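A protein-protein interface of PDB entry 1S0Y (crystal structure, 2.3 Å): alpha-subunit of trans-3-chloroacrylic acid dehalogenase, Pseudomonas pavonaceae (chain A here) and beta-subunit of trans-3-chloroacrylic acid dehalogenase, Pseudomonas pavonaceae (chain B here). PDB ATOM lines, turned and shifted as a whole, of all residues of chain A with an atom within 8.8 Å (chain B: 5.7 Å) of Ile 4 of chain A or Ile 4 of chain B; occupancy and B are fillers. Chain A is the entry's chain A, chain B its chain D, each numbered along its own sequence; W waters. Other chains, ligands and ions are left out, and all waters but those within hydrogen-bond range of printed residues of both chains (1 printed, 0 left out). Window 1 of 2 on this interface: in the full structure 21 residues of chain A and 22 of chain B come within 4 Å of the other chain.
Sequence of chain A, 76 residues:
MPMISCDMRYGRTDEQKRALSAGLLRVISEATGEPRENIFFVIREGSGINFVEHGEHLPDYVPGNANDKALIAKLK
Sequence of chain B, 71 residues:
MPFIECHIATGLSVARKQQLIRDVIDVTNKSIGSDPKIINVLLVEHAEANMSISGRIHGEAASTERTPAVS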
ATOM      1  N   PRO A   2      15.217  -3.832 -13.758  1.00  0.00           N
ATOM      2  CA  PRO A   2      16.180  -2.863 -14.318  1.00  0.00           C
ATOM      3  C   PRO A   2      15.685  -1.430 -14.172  1.00  0.00           C
ATOM      4  O   PRO A   2      14.478  -1.193 -14.088  1.00  0.00           O
ATOM      5  CB  PRO A   2      16.375  -3.227 -15.786  1.00  0.00           C
ATOM      6  CG  PRO A   2      15.087  -3.983 -16.092  1.00  0.00           C
ATOM      7  CD  PRO A   2      14.808  -4.779 -14.810  1.00  0.00           C
ATOM      8  N   MET A   3      16.626  -0.487 -14.122  1.00  0.00           N
ATOM      9  CA  MET A   3      16.294   0.932 -13.996  1.00  0.00           C
ATOM     10  C   MET A   3      16.719   1.665 -15.247  1.00  0.00           C
ATOM     11  O   MET A   3      17.826   1.469 -15.751  1.00  0.00           O
ATOM     12  CB  MET A   3      17.001   1.587 -12.805  1.00  0.00           C
ATOM     13  CG  MET A   3      16.653   1.021 -11.451  1.00  0.00           C
ATOM     14  SD  MET A   3      17.644  -0.407 -11.059  1.00  0.00           S
ATOM     15  CE  MET A   3      17.143  -0.703  -9.354  1.00  0.00           C
ATOM     16  N   ILE A   4      15.834   2.520 -15.741  1.00  0.00           N
ATOM     17  CA  ILE A   4      16.117   3.300 -16.931  1.00  0.00           C
ATOM     18  C   ILE A   4      15.847   4.768 -16.657  1.00  0.00           C
ATOM     19  O   ILE A   4      14.860   5.118 -16.007  1.00  0.00           O
ATOM     20  CB  ILE A   4      15.231   2.861 -18.107  1.00  0.00           C
ATOM     21  CG1 ILE A   4      15.381   1.355 -18.324  1.00  0.00           C
ATOM     22  CG2 ILE A   4      15.619   3.635 -19.362  1.00  0.00           C
ATOM     23  CD1 ILE A   4      14.515   0.818 -19.427  1.00  0.00           C
ATOM     24  N   SER A   5      16.732   5.624 -17.156  1.00  0.00           N
ATOM     25  CA  SER A   5      16.577   7.059 -16.988  1.00  0.00           C
ATOM     26  C   SER A   5      16.740   7.717 -18.342  1.00  0.00           C
ATOM     27  O   SER A   5      17.530   7.266 -19.169  1.00  0.00           O
ATOM     28  CB  SER A   5      17.625   7.616 -16.017  1.00  0.00           C
ATOM     29  OG  SER A   5      18.944   7.503 -16.533  1.00  0.00           O
ATOM     30  N   CYS A   6      15.976   8.776 -18.571  1.00  0.00           N
ATOM     31  CA  CYS A   6      16.070   9.507 -19.819  1.00  0.00           C
ATOM     32  C   CYS A   6      16.132  11.004 -19.560  1.00  0.00           C
ATOM     33  O   CYS A   6      15.131  11.623 -19.215  1.00  0.00           O
ATOM     34  CB  CYS A   6      14.879   9.203 -20.719  1.00  0.00           C
ATOM     35  SG  CYS A   6      14.829  10.302 -22.152  1.00  0.00           S
ATOM     36  N   ASP A   7      17.322  11.566 -19.725  1.00  0.00           N
ATOM     37  CA  ASP A   7      17.572  12.995 -19.533  1.00  0.00           C
ATOM     38  C   ASP A   7      17.246  13.755 -20.813  1.00  0.00           C
ATOM     39  O   ASP A   7      18.014  13.709 -21.762  1.00  0.00           O
ATOM     40  CB  ASP A   7      19.051  13.219 -19.219  1.00  0.00           C
ATOM     41  CG  ASP A   7      19.360  13.172 -17.740  1.00  0.00           C
ATOM     42  OD1 ASP A   7      19.357  14.250 -17.111  1.00  0.00           O
ATOM     43  OD2 ASP A   7      19.615  12.061 -17.215  1.00  0.00           O
ATOM     44  N   MET A   8      16.124  14.459 -20.857  1.00  0.00           N
ATOM     45  CA  MET A   8      15.812  15.201 -22.073  1.00  0.00           C
ATOM     46  C   MET A   8      15.273  16.592 -21.784  1.00  0.00           C
ATOM     47  O   MET A   8      14.839  16.867 -20.674  1.00  0.00           O
ATOM     48  CB  MET A   8      14.829  14.417 -22.951  1.00  0.00           C
ATOM     49  CG  MET A   8      13.415  14.334 -22.445  1.00  0.00           C
ATOM     50  SD  MET A   8      12.466  13.271 -23.547  1.00  0.00           S
ATOM     51  CE  MET A   8      10.885  13.109 -22.598  1.00  0.00           C
ATOM     52  N   LEU A  20       6.953   6.941 -25.028  1.00  0.00           N
ATOM     53  CA  LEU A  20       8.367   6.701 -24.790  1.00  0.00           C
ATOM     54  C   LEU A  20       8.538   5.547 -23.805  1.00  0.00           C
ATOM     55  O   LEU A  20       9.263   4.587 -24.078  1.00  0.00           O
ATOM     56  CB  LEU A  20       9.029   7.955 -24.227  1.00  0.00           C
ATOM     57  CG  LEU A  20      10.523   7.823 -23.929  1.00  0.00           C
ATOM     58  CD1 LEU A  20      11.265   7.520 -25.217  1.00  0.00           C
ATOM     59  CD2 LEU A  20      11.035   9.106 -23.307  1.00  0.00           C
ATOM     60  N   SER A  21       7.855   5.637 -22.666  1.00  0.00           N
ATOM     61  CA  SER A  21       7.943   4.601 -21.641  1.00  0.00           C
ATOM     62  C   SER A  21       7.421   3.258 -22.140  1.00  0.00           C
ATOM     63  O   SER A  21       8.022   2.214 -21.884  1.00  0.00           O
ATOM     64  CB  SER A  21       7.170   5.024 -20.392  1.00  0.00           C
ATOM     65  OG  SER A  21       5.831   5.333 -20.716  1.00  0.00           O
ATOM     66  N   GLY A  23       7.445   2.153 -25.059  1.00  0.00           N
ATOM     67  CA  GLY A  23       8.447   1.608 -25.955  1.00  0.00           C
ATOM     68  C   GLY A  23       9.742   1.221 -25.266  1.00  0.00           C
ATOM     69  O   GLY A  23      10.310   0.167 -25.543  1.00  0.00           O
ATOM     70  N   LEU A  24      10.216   2.074 -24.369  1.00  0.00           N
ATOM     71  CA  LEU A  24      11.448   1.793 -23.645  1.00  0.00           C
ATOM     72  C   LEU A  24      11.304   0.531 -22.791  1.00  0.00           C
ATOM     73  O   LEU A  24      12.195  -0.319 -22.772  1.00  0.00           O
ATOM     74  CB  LEU A  24      11.821   2.994 -22.778  1.00  0.00           C
ATOM     75  CG  LEU A  24      13.081   3.767 -23.174  1.00  0.00           C
ATOM     76  CD1 LEU A  24      13.220   3.855 -24.670  1.00  0.00           C
ATOM     77  CD2 LEU A  24      13.031   5.150 -22.568  1.00  0.00           C
ATOM     78  N   LEU A  25      10.185   0.400 -22.087  1.00  0.00           N
ATOM     79  CA  LEU A  25       9.983  -0.787 -21.269  1.00  0.00           C
ATOM     80  C   LEU A  25       9.848  -2.048 -22.123  1.00  0.00           C
ATOM     81  O   LEU A  25      10.329  -3.113 -21.742  1.00  0.00           O
ATOM     82  CB  LEU A  25       8.756  -0.629 -20.368  1.00  0.00           C
ATOM     83  CG  LEU A  25       9.057   0.009 -19.006  1.00  0.00           C
ATOM     84  CD1 LEU A  25       9.506   1.448 -19.196  1.00  0.00           C
ATOM     85  CD2 LEU A  25       7.825  -0.041 -18.129  1.00  0.00           C
ATOM     86  N   ARG A  26       9.218  -1.936 -23.286  1.00  0.00           N
ATOM     87  CA  ARG A  26       9.059  -3.105 -24.140  1.00  0.00           C
ATOM     88  C   ARG A  26      10.401  -3.677 -24.600  1.00  0.00           C
ATOM     89  O   ARG A  26      10.681  -4.851 -24.374  1.00  0.00           O
ATOM     90  CB  ARG A  26       8.211  -2.766 -25.365  1.00  0.00           C
ATOM     91  CG  ARG A  26       7.891  -3.975 -26.245  1.00  0.00           C
ATOM     92  CD  ARG A  26       7.481  -3.529 -27.626  1.00  0.00           C
ATOM     93  NE  ARG A  26       8.529  -2.708 -28.224  1.00  0.00           N
ATOM     94  CZ  ARG A  26       8.428  -2.087 -29.394  1.00  0.00           C
ATOM     95  NH1 ARG A  26       7.316  -2.188 -30.112  1.00  0.00           N
ATOM     96  NH2 ARG A  26       9.439  -1.355 -29.843  1.00  0.00           N
ATOM     97  N   VAL A  27      11.227  -2.854 -25.240  1.00  0.00           N
ATOM     98  CA  VAL A  27      12.521  -3.317 -25.735  1.00  0.00           C
ATOM     99  C   VAL A  27      13.438  -3.815 -24.628  1.00  0.00           C
ATOM    100  O   VAL A  27      14.232  -4.738 -24.840  1.00  0.00           O
ATOM    101  CB  VAL A  27      13.266  -2.215 -26.524  1.00  0.00           C
ATOM    102  CG1 VAL A  27      12.420  -1.761 -27.711  1.00  0.00           C
ATOM    103  CG2 VAL A  27      13.587  -1.047 -25.618  1.00  0.00           C
ATOM    104  N   ILE A  28      13.329  -3.210 -23.446  1.00  0.00           N
ATOM    105  CA  ILE A  28      14.161  -3.613 -22.318  1.00  0.00           C
ATOM    106  C   ILE A  28      13.693  -4.937 -21.749  1.00  0.00           C
ATOM    107  O   ILE A  28      14.504  -5.802 -21.413  1.00  0.00           O
ATOM    108  CB  ILE A  28      14.148  -2.553 -21.203  1.00  0.00           C
ATOM    109  CG1 ILE A  28      15.052  -1.382 -21.597  1.00  0.00           C
ATOM    110  CG2 ILE A  28      14.600  -3.167 -19.884  1.00  0.00           C
ATOM    111  CD1 ILE A  28      16.539  -1.710 -21.648  1.00  0.00           C
ATOM    112  N   SER A  29      12.379  -5.090 -21.638  1.00  0.00           N
ATOM    113  CA  SER A  29      11.798  -6.320 -21.116  1.00  0.00           C
ATOM    114  C   SER A  29      12.015  -7.422 -22.139  1.00  0.00           C
ATOM    115  O   SER A  29      12.135  -8.597 -21.799  1.00  0.00           O
ATOM    116  CB  SER A  29      10.301  -6.137 -20.875  1.00  0.00           C
ATOM    117  OG  SER A  29       9.687  -7.385 -20.619  1.00  0.00           O
ATOM    118  N   THR A  32      15.769  -8.281 -21.880  1.00  0.00           N
ATOM    119  CA  THR A  32      16.092  -8.751 -20.535  1.00  0.00           C
ATOM    120  C   THR A  32      15.228  -9.941 -20.103  1.00  0.00           C
ATOM    121  O   THR A  32      15.607 -10.703 -19.206  1.00  0.00           O
ATOM    122  CB  THR A  32      15.900  -7.626 -19.493  1.00  0.00           C
ATOM    123  OG1 THR A  32      16.819  -6.558 -19.762  1.00  0.00           O
ATOM    124  CG2 THR A  32      16.150  -8.146 -18.094  1.00  0.00           C
ATOM    125  N   ASN A  38       8.770  -5.152 -13.329  1.00  0.00           N
ATOM    126  CA  ASN A  38      10.105  -5.198 -12.744  1.00  0.00           C
ATOM    127  C   ASN A  38      11.053  -4.187 -13.400  1.00  0.00           C
ATOM    128  O   ASN A  38      12.275  -4.308 -13.323  1.00  0.00           O
ATOM    129  CB  ASN A  38      10.670  -6.609 -12.861  1.00  0.00           C
ATOM    130  N   ILE A  39      10.477  -3.179 -14.041  1.00  0.00           N
ATOM    131  CA  ILE A  39      11.268  -2.150 -14.702  1.00  0.00           C
ATOM    132  C   ILE A  39      10.952  -0.793 -14.108  1.00  0.00           C
ATOM    133  O   ILE A  39       9.792  -0.483 -13.833  1.00  0.00           O
ATOM    134  CB  ILE A  39      10.945  -2.072 -16.199  1.00  0.00           C
ATOM    135  CG1 ILE A  39      11.124  -3.448 -16.845  1.00  0.00           C
ATOM    136  CG2 ILE A  39      11.820  -1.024 -16.854  1.00  0.00           C
ATOM    137  CD1 ILE A  39      10.654  -3.521 -18.281  1.00  0.00           C
ATOM    138  N   PHE A  40      11.980   0.018 -13.898  1.00  0.00           N
ATOM    139  CA  PHE A  40      11.756   1.358 -13.374  1.00  0.00           C
ATOM    140  C   PHE A  40      12.251   2.350 -14.407  1.00  0.00           C
ATOM    141  O   PHE A  40      13.288   2.136 -15.034  1.00  0.00           O
ATOM    142  CB  PHE A  40      12.498   1.585 -12.057  1.00  0.00           C
ATOM    143  CG  PHE A  40      12.430   3.007 -11.578  1.00  0.00           C
ATOM    144  CD1 PHE A  40      11.215   3.572 -11.218  1.00  0.00           C
ATOM    145  CD2 PHE A  40      13.574   3.799 -11.542  1.00  0.00           C
ATOM    146  CE1 PHE A  40      11.139   4.909 -10.833  1.00  0.00           C
ATOM    147  CE2 PHE A  40      13.507   5.136 -11.159  1.00  0.00           C
ATOM    148  CZ  PHE A  40      12.291   5.691 -10.806  1.00  0.00           C
ATOM    149  N   PHE A  41      11.510   3.436 -14.588  1.00  0.00           N
ATOM    150  CA  PHE A  41      11.892   4.444 -15.563  1.00  0.00           C
ATOM    151  C   PHE A  41      11.673   5.855 -15.040  1.00  0.00           C
ATOM    152  O   PHE A  41      10.659   6.154 -14.420  1.00  0.00           O
ATOM    153  CB  PHE A  41      11.111   4.233 -16.863  1.00  0.00           C
ATOM    154  CG  PHE A  41      11.354   5.297 -17.903  1.00  0.00           C
ATOM    155  CD1 PHE A  41      12.654   5.653 -18.275  1.00  0.00           C
ATOM    156  CD2 PHE A  41      10.282   5.928 -18.534  1.00  0.00           C
ATOM    157  CE1 PHE A  41      12.879   6.614 -19.258  1.00  0.00           C
ATOM    158  CE2 PHE A  41      10.500   6.895 -19.523  1.00  0.00           C
ATOM    159  CZ  PHE A  41      11.803   7.235 -19.885  1.00  0.00           C
ATOM    160  N   VAL A  42      12.638   6.726 -15.280  1.00  0.00           N
ATOM    161  CA  VAL A  42      12.513   8.100 -14.825  1.00  0.00           C
ATOM    162  C   VAL A  42      13.018   9.065 -15.883  1.00  0.00           C
ATOM    163  O   VAL A  42      14.053   8.835 -16.509  1.00  0.00           O
ATOM    164  CB  VAL A  42      13.275   8.324 -13.498  1.00  0.00           C
ATOM    165  CG1 VAL A  42      14.704   7.824 -13.617  1.00  0.00           C
ATOM    166  CG2 VAL A  42      13.242   9.797 -13.128  1.00  0.00           C
ATOM    167  N   ILE A  43      12.251  10.132 -16.084  1.00  0.00           N
ATOM    168  CA  ILE A  43      12.576  11.176 -17.045  1.00  0.00           C
ATOM    169  C   ILE A  43      13.059  12.441 -16.312  1.00  0.00           C
ATOM    170  O   ILE A  43      12.358  12.978 -15.452  1.00  0.00           O
ATOM    171  CB  ILE A  43      11.323  11.531 -17.890  1.00  0.00           C
ATOM    172  CG1 ILE A  43      10.881  10.313 -18.694  1.00  0.00           C
ATOM    173  CG2 ILE A  43      11.627  12.694 -18.829  1.00  0.00           C
ATOM    174  CD1 ILE A  43       9.382  10.267 -18.947  1.00  0.00           C
ATOM    175  N   ARG A  44      14.263  12.897 -16.640  1.00  0.00           N
ATOM    176  CA  ARG A  44      14.806  14.113 -16.042  1.00  0.00           C
ATOM    177  C   ARG A  44      14.763  15.189 -17.127  1.00  0.00           C
ATOM    178  O   ARG A  44      15.124  14.932 -18.280  1.00  0.00           O
ATOM    179  CB  ARG A  44      16.245  13.890 -15.581  1.00  0.00           C
ATOM    180  CG  ARG A  44      16.379  12.847 -14.490  1.00  0.00           C
ATOM    181  CD  ARG A  44      17.833  12.644 -14.129  1.00  0.00           C
ATOM    182  NE  ARG A  44      18.019  11.522 -13.217  1.00  0.00           N
ATOM    183  CZ  ARG A  44      18.770  10.464 -13.502  1.00  0.00           C
ATOM    184  NH1 ARG A  44      19.395  10.397 -14.671  1.00  0.00           N
ATOM    185  NH2 ARG A  44      18.897   9.476 -12.625  1.00  0.00           N
ATOM    186  N   PHE A  51      21.561  21.217 -22.464  1.00  0.00           N
ATOM    187  CA  PHE A  51      21.870  20.057 -23.291  1.00  0.00           C
ATOM    188  C   PHE A  51      22.863  20.399 -24.383  1.00  0.00           C
ATOM    189  O   PHE A  51      22.538  21.111 -25.333  1.00  0.00           O
ATOM    190  CB  PHE A  51      20.596  19.489 -23.905  1.00  0.00           C
ATOM    191  CG  PHE A  51      19.795  18.670 -22.955  1.00  0.00           C
ATOM    192  CD1 PHE A  51      19.138  19.269 -21.889  1.00  0.00           C
ATOM    193  CD2 PHE A  51      19.740  17.281 -23.088  1.00  0.00           C
ATOM    194  CE1 PHE A  51      18.439  18.496 -20.963  1.00  0.00           C
ATOM    195  CE2 PHE A  51      19.047  16.502 -22.172  1.00  0.00           C
ATOM    196  CZ  PHE A  51      18.395  17.109 -21.104  1.00  0.00           C
ATOM    197  N   PRO B   2      17.481  13.364 -25.974  1.00  0.00           N
ATOM    198  CA  PRO B   2      17.477  12.253 -25.017  1.00  0.00           C
ATOM    199  C   PRO B   2      18.793  11.532 -24.770  1.00  0.00           C
ATOM    200  O   PRO B   2      19.497  11.137 -25.707  1.00  0.00           O
ATOM    201  CB  PRO B   2      16.379  11.326 -25.536  1.00  0.00           C
ATOM    202  CG  PRO B   2      16.271  11.656 -26.962  1.00  0.00           C
ATOM    203  CD  PRO B   2      16.524  13.119 -27.069  1.00  0.00           C
ATOM    204  N   PHE B   3      19.124  11.402 -23.491  1.00  0.00           N
ATOM    205  CA  PHE B   3      20.321  10.691 -23.033  1.00  0.00           C
ATOM    206  C   PHE B   3      19.726   9.623 -22.136  1.00  0.00           C
ATOM    207  O   PHE B   3      19.319   9.899 -21.008  1.00  0.00           O
ATOM    208  CB  PHE B   3      21.240  11.605 -22.219  1.00  0.00           C
ATOM    209  CG  PHE B   3      22.274  10.864 -21.416  1.00  0.00           C
ATOM    210  CD1 PHE B   3      22.996   9.816 -21.978  1.00  0.00           C
ATOM    211  CD2 PHE B   3      22.525  11.212 -20.093  1.00  0.00           C
ATOM    212  CE1 PHE B   3      23.950   9.122 -21.238  1.00  0.00           C
ATOM    213  CE2 PHE B   3      23.478  10.528 -19.342  1.00  0.00           C
ATOM    214  CZ  PHE B   3      24.194   9.477 -19.917  1.00  0.00           C
ATOM    215  N   ILE B   4      19.646   8.410 -22.664  1.00  0.00           N
ATOM    216  CA  ILE B   4      19.061   7.294 -21.952  1.00  0.00           C
ATOM    217  C   ILE B   4      20.125   6.424 -21.320  1.00  0.00           C
ATOM    218  O   ILE B   4      21.138   6.108 -21.953  1.00  0.00           O
ATOM    219  CB  ILE B   4      18.216   6.450 -22.925  1.00  0.00           C
ATOM    220  CG1 ILE B   4      17.214   7.366 -23.641  1.00  0.00           C
ATOM    221  CG2 ILE B   4      17.502   5.339 -22.175  1.00  0.00           C
ATOM    222  CD1 ILE B   4      16.554   6.740 -24.857  1.00  0.00           C
ATOM    223  N   GLU B   5      19.909   6.049 -20.063  1.00  0.00           N
ATOM    224  CA  GLU B   5      20.861   5.186 -19.366  1.00  0.00           C
ATOM    225  C   GLU B   5      20.104   3.964 -18.871  1.00  0.00           C
ATOM    226  O   GLU B   5      19.175   4.074 -18.075  1.00  0.00           O
ATOM    227  CB  GLU B   5      21.521   5.934 -18.201  1.00  0.00           C
ATOM    228  CG  GLU B   5      22.629   5.155 -17.513  1.00  0.00           C
ATOM    229  CD  GLU B   5      23.491   6.016 -16.600  1.00  0.00           C
ATOM    230  OE1 GLU B   5      24.358   5.454 -15.897  1.00  0.00           O
ATOM    231  OE2 GLU B   5      23.309   7.253 -16.593  1.00  0.00           O
ATOM    232  N   CYS B   6      20.494   2.793 -19.357  1.00  0.00           N
ATOM    233  CA  CYS B   6      19.816   1.562 -18.970  1.00  0.00           C
ATOM    234  C   CYS B   6      20.640   0.724 -18.018  1.00  0.00           C
ATOM    235  O   CYS B   6      21.761   0.335 -18.330  1.00  0.00           O
ATOM    236  CB  CYS B   6      19.492   0.729 -20.205  1.00  0.00           C
ATOM    237  SG  CYS B   6      18.591   1.619 -21.478  1.00  0.00           S
ATOM    238  N   HIS B   7      20.071   0.445 -16.853  1.00  0.00           N
ATOM    239  CA  HIS B   7      20.741  -0.368 -15.858  1.00  0.00           C
ATOM    240  C   HIS B   7      20.076  -1.733 -15.851  1.00  0.00           C
ATOM    241  O   HIS B   7      18.901  -1.852 -15.510  1.00  0.00           O
ATOM    242  CB  HIS B   7      20.622   0.294 -14.488  1.00  0.00           C
ATOM    243  CG  HIS B   7      21.309   1.617 -14.413  1.00  0.00           C
ATOM    244  ND1 HIS B   7      22.675   1.738 -14.267  1.00  0.00           N
ATOM    245  CD2 HIS B   7      20.829   2.879 -14.519  1.00  0.00           C
ATOM    246  CE1 HIS B   7      23.005   3.017 -14.286  1.00  0.00           C
ATOM    247  NE2 HIS B   7      21.904   3.731 -14.438  1.00  0.00           N
ATOM    248  N   VAL B  24      16.596   0.799 -28.507  1.00  0.00           N
ATOM    249  CA  VAL B  24      16.243   1.981 -27.721  1.00  0.00           C
ATOM    250  C   VAL B  24      16.336   3.258 -28.553  1.00  0.00           C
ATOM    251  O   VAL B  24      15.502   4.149 -28.416  1.00  0.00           O
ATOM    252  CB  VAL B  24      17.132   2.129 -26.466  1.00  0.00           C
ATOM    253  CG1 VAL B  24      16.935   0.935 -25.558  1.00  0.00           C
ATOM    254  CG2 VAL B  24      18.584   2.245 -26.862  1.00  0.00           C
ATOM    255  N   THR B  28      12.860   5.372 -29.332  1.00  0.00           N
ATOM    256  CA  THR B  28      12.836   6.755 -28.881  1.00  0.00           C
ATOM    257  C   THR B  28      12.477   7.625 -30.070  1.00  0.00           C
ATOM    258  O   THR B  28      11.514   8.394 -30.031  1.00  0.00           O
ATOM    259  CB  THR B  28      14.211   7.194 -28.358  1.00  0.00           C
ATOM    260  OG1 THR B  28      14.516   6.475 -27.161  1.00  0.00           O
ATOM    261  CG2 THR B  28      14.226   8.686 -28.079  1.00  0.00           C
ATOM    262  N   ILE B  39      20.396  11.412 -30.047  1.00  0.00           N
ATOM    263  CA  ILE B  39      20.023  10.380 -29.083  1.00  0.00           C
ATOM    264  C   ILE B  39      21.323   9.764 -28.588  1.00  0.00           C
ATOM    265  O   ILE B  39      22.177   9.392 -29.389  1.00  0.00           O
ATOM    266  CB  ILE B  39      19.183   9.235 -29.694  1.00  0.00           C
ATOM    267  CG1 ILE B  39      17.732   9.669 -29.925  1.00  0.00           C
ATOM    268  CG2 ILE B  39      19.177   8.054 -28.731  1.00  0.00           C
ATOM    269  CD1 ILE B  39      17.583  10.893 -30.746  1.00  0.00           C
ATOM    270  N   ASN B  40      21.480   9.672 -27.271  1.00  0.00           N
ATOM    271  CA  ASN B  40      22.682   9.084 -26.700  1.00  0.00           C
ATOM    272  C   ASN B  40      22.267   8.015 -25.714  1.00  0.00           C
ATOM    273  O   ASN B  40      21.472   8.270 -24.808  1.00  0.00           O
ATOM    274  CB  ASN B  40      23.519  10.148 -25.999  1.00  0.00           C
ATOM    275  CG  ASN B  40      24.109  11.138 -26.964  1.00  0.00           C
ATOM    276  OD1 ASN B  40      25.020  10.811 -27.721  1.00  0.00           O
ATOM    277  ND2 ASN B  40      23.584  12.357 -26.956  1.00  0.00           N
ATOM    278  N   VAL B  41      22.812   6.817 -25.896  1.00  0.00           N
ATOM    279  CA  VAL B  41      22.467   5.700 -25.033  1.00  0.00           C
ATOM    280  C   VAL B  41      23.667   5.136 -24.281  1.00  0.00           C
ATOM    281  O   VAL B  41      24.781   5.090 -24.802  1.00  0.00           O
ATOM    282  CB  VAL B  41      21.788   4.589 -25.860  1.00  0.00           C
ATOM    283  CG1 VAL B  41      21.250   3.485 -24.946  1.00  0.00           C
ATOM    284  CG2 VAL B  41      20.655   5.197 -26.683  1.00  0.00           C
ATOM    285  N   LEU B  42      23.427   4.726 -23.040  1.00  0.00           N
ATOM    286  CA  LEU B  42      24.469   4.161 -22.194  1.00  0.00           C
ATOM    287  C   LEU B  42      23.897   2.924 -21.515  1.00  0.00           C
ATOM    288  O   LEU B  42      22.887   2.996 -20.804  1.00  0.00           O
ATOM    289  CB  LEU B  42      24.909   5.178 -21.134  1.00  0.00           C
ATOM    290  CG  LEU B  42      26.319   5.036 -20.543  1.00  0.00           C
ATOM    291  CD1 LEU B  42      26.521   6.124 -19.488  1.00  0.00           C
ATOM    292  CD2 LEU B  42      26.524   3.652 -19.939  1.00  0.00           C
ATOM    293  N   LEU B  43      24.540   1.790 -21.744  1.00  0.00           N
ATOM    294  CA  LEU B  43      24.098   0.530 -21.170  1.00  0.00           C
ATOM    295  C   LEU B  43      25.094   0.138 -20.101  1.00  0.00           C
ATOM    296  O   LEU B  43      26.292   0.080 -20.362  1.00  0.00           O
ATOM    297  CB  LEU B  43      24.047  -0.547 -22.254  1.00  0.00           C
ATOM    298  CG  LEU B  43      23.721  -1.978 -21.822  1.00  0.00           C
ATOM    299  CD1 LEU B  43      22.332  -2.024 -21.181  1.00  0.00           C
ATOM    300  CD2 LEU B  43      23.785  -2.903 -23.047  1.00  0.00           C
HETATM  301  O   HOH W   1      19.582   9.247 -18.345  1.00  0.00           O
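Among the printed residues, pairs that only touch across the chains: Pro 2 of chain A with His 7 of chain B (2.9 Å), Met 3 of chain A with Glu 5 of chain B (3.7 Å), Met 3 of chain A with Cys 6 of chain B (3.7 Å), Ile 4 of chain A with Ile 4 of chain B (3.8 Å), Ile 4 of chain A with Glu 5 of chain B (3.4 Å), Ser 5 of chain A with Phe 3 of chain B (3.7 Å), Ser 5 of chain A with Ile 4 of chain B (3.2 Å), Cys 6 of chain A with Pro 2 of chain B (3.9 Å), Cys 6 of chain A with Phe 3 of chain B (3.5 Å), Asp 7 of chain A with Pro 2 of chain B (3.6 Å), Met 8 of chain A with Pro 2 of chain B (3.995 Å), Leu 20 of chain A with Thr 28 of chain B (3.9 Å), Leu 24 of chain A with Thr 28 of chain B (3.8 Å), Val 27 of chain A with Val 24 of chain B (3.9 Å) and Ile 28 of chain A with Cys 6 of chain B (3.9 Å).
Water W1 lies within hydrogen-bond range of OG of Ser 5 of chain A (2.6 Å), O of Phe 3 of chain B (2.8 Å) and OD2 of Asp 7 of chain A (3.0 Å).
The backbone NH (N) of Glu 5 of chain B sits at hydrogen-bond distance from the backbone carbonyl oxygen (O) of Ser 5 of chain A, 2.8 Å away.
The backbone NH (N) of Asp 7 of chain A lies within hydrogen-bond range of the backbone carbonyl oxygen (O) of Phe 3 of chain B, 2.9 Å away.
The backbone carbonyl oxygen of Met 3 of chain A is in hydrogen-bond range of the backbone NH of His 7 of chain B.
N of Arg 44 of chain A lies within hydrogen-bond range of O of Cys 6 of chain A (3.0 Å).
N of Asn 40 of chain B is in hydrogen-bond range of O of Pro 2 of chain B (2.9 Å).
OE1 of Glu 5 of chain B lies close to NE2 of His 7 of chain B, at 3.3 Å.
N of Met 8 of chain A is in hydrogen-bond range of O of Arg 44 of chain A, 2.8 Å away.
O of Ile 4 of chain B lies within hydrogen-bond range of N of Leu 42 of chain B (2.9 Å).
O of Val 24 of chain B lies within hydrogen-bond range of OG1 of Thr 28 of chain B, at 2.8 Å.
Printed residues of chain B within 4 Å of Pro 2 of chain A: His 7 (2.9 Å).
Of chain B, only Ile 4 (3.8 Å) and Glu 5 (3.4 Å) come within 4 Å of Ile 4 of chain A.
Of the printed residues of chain B, Leu 20 of chain A touches Thr 28 (3.9 Å).
Ser 21 of chain A touches none of the printed residues of chain B.
Printed residues of chain B within 4 Å of Leu 24 of chain A: Thr 28.
Printed residues of chain A within 4 Å of Phe 3 of chain B: Ser 5, Cys 6 and Asp 7.
Of chain A, only Ile 4 (3.8 Å) and Ser 5 (3.2 Å) come within 4 Å of Ile 4 of chain B.
Of the printed residues of chain A, Cys 6 of chain B touches Met 3 (3.7 Å) and Ile 28 (3.9 Å).
The nearest residue of chain A that does not touch Ile 4 of chain B is Cys 6 of chain A (4.1 Å).
Of the 13 printed residues of chain B, 8 touch a printed residue of chain A.
Hydrophobic or aromatic side chains of chain B that line the printed part of chain A: Pro 2, Phe 3, Ile 4, His 7 and Val 24.
Along chain B the printed residues that touch a printed residue of chain A span positions 2 to 28.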
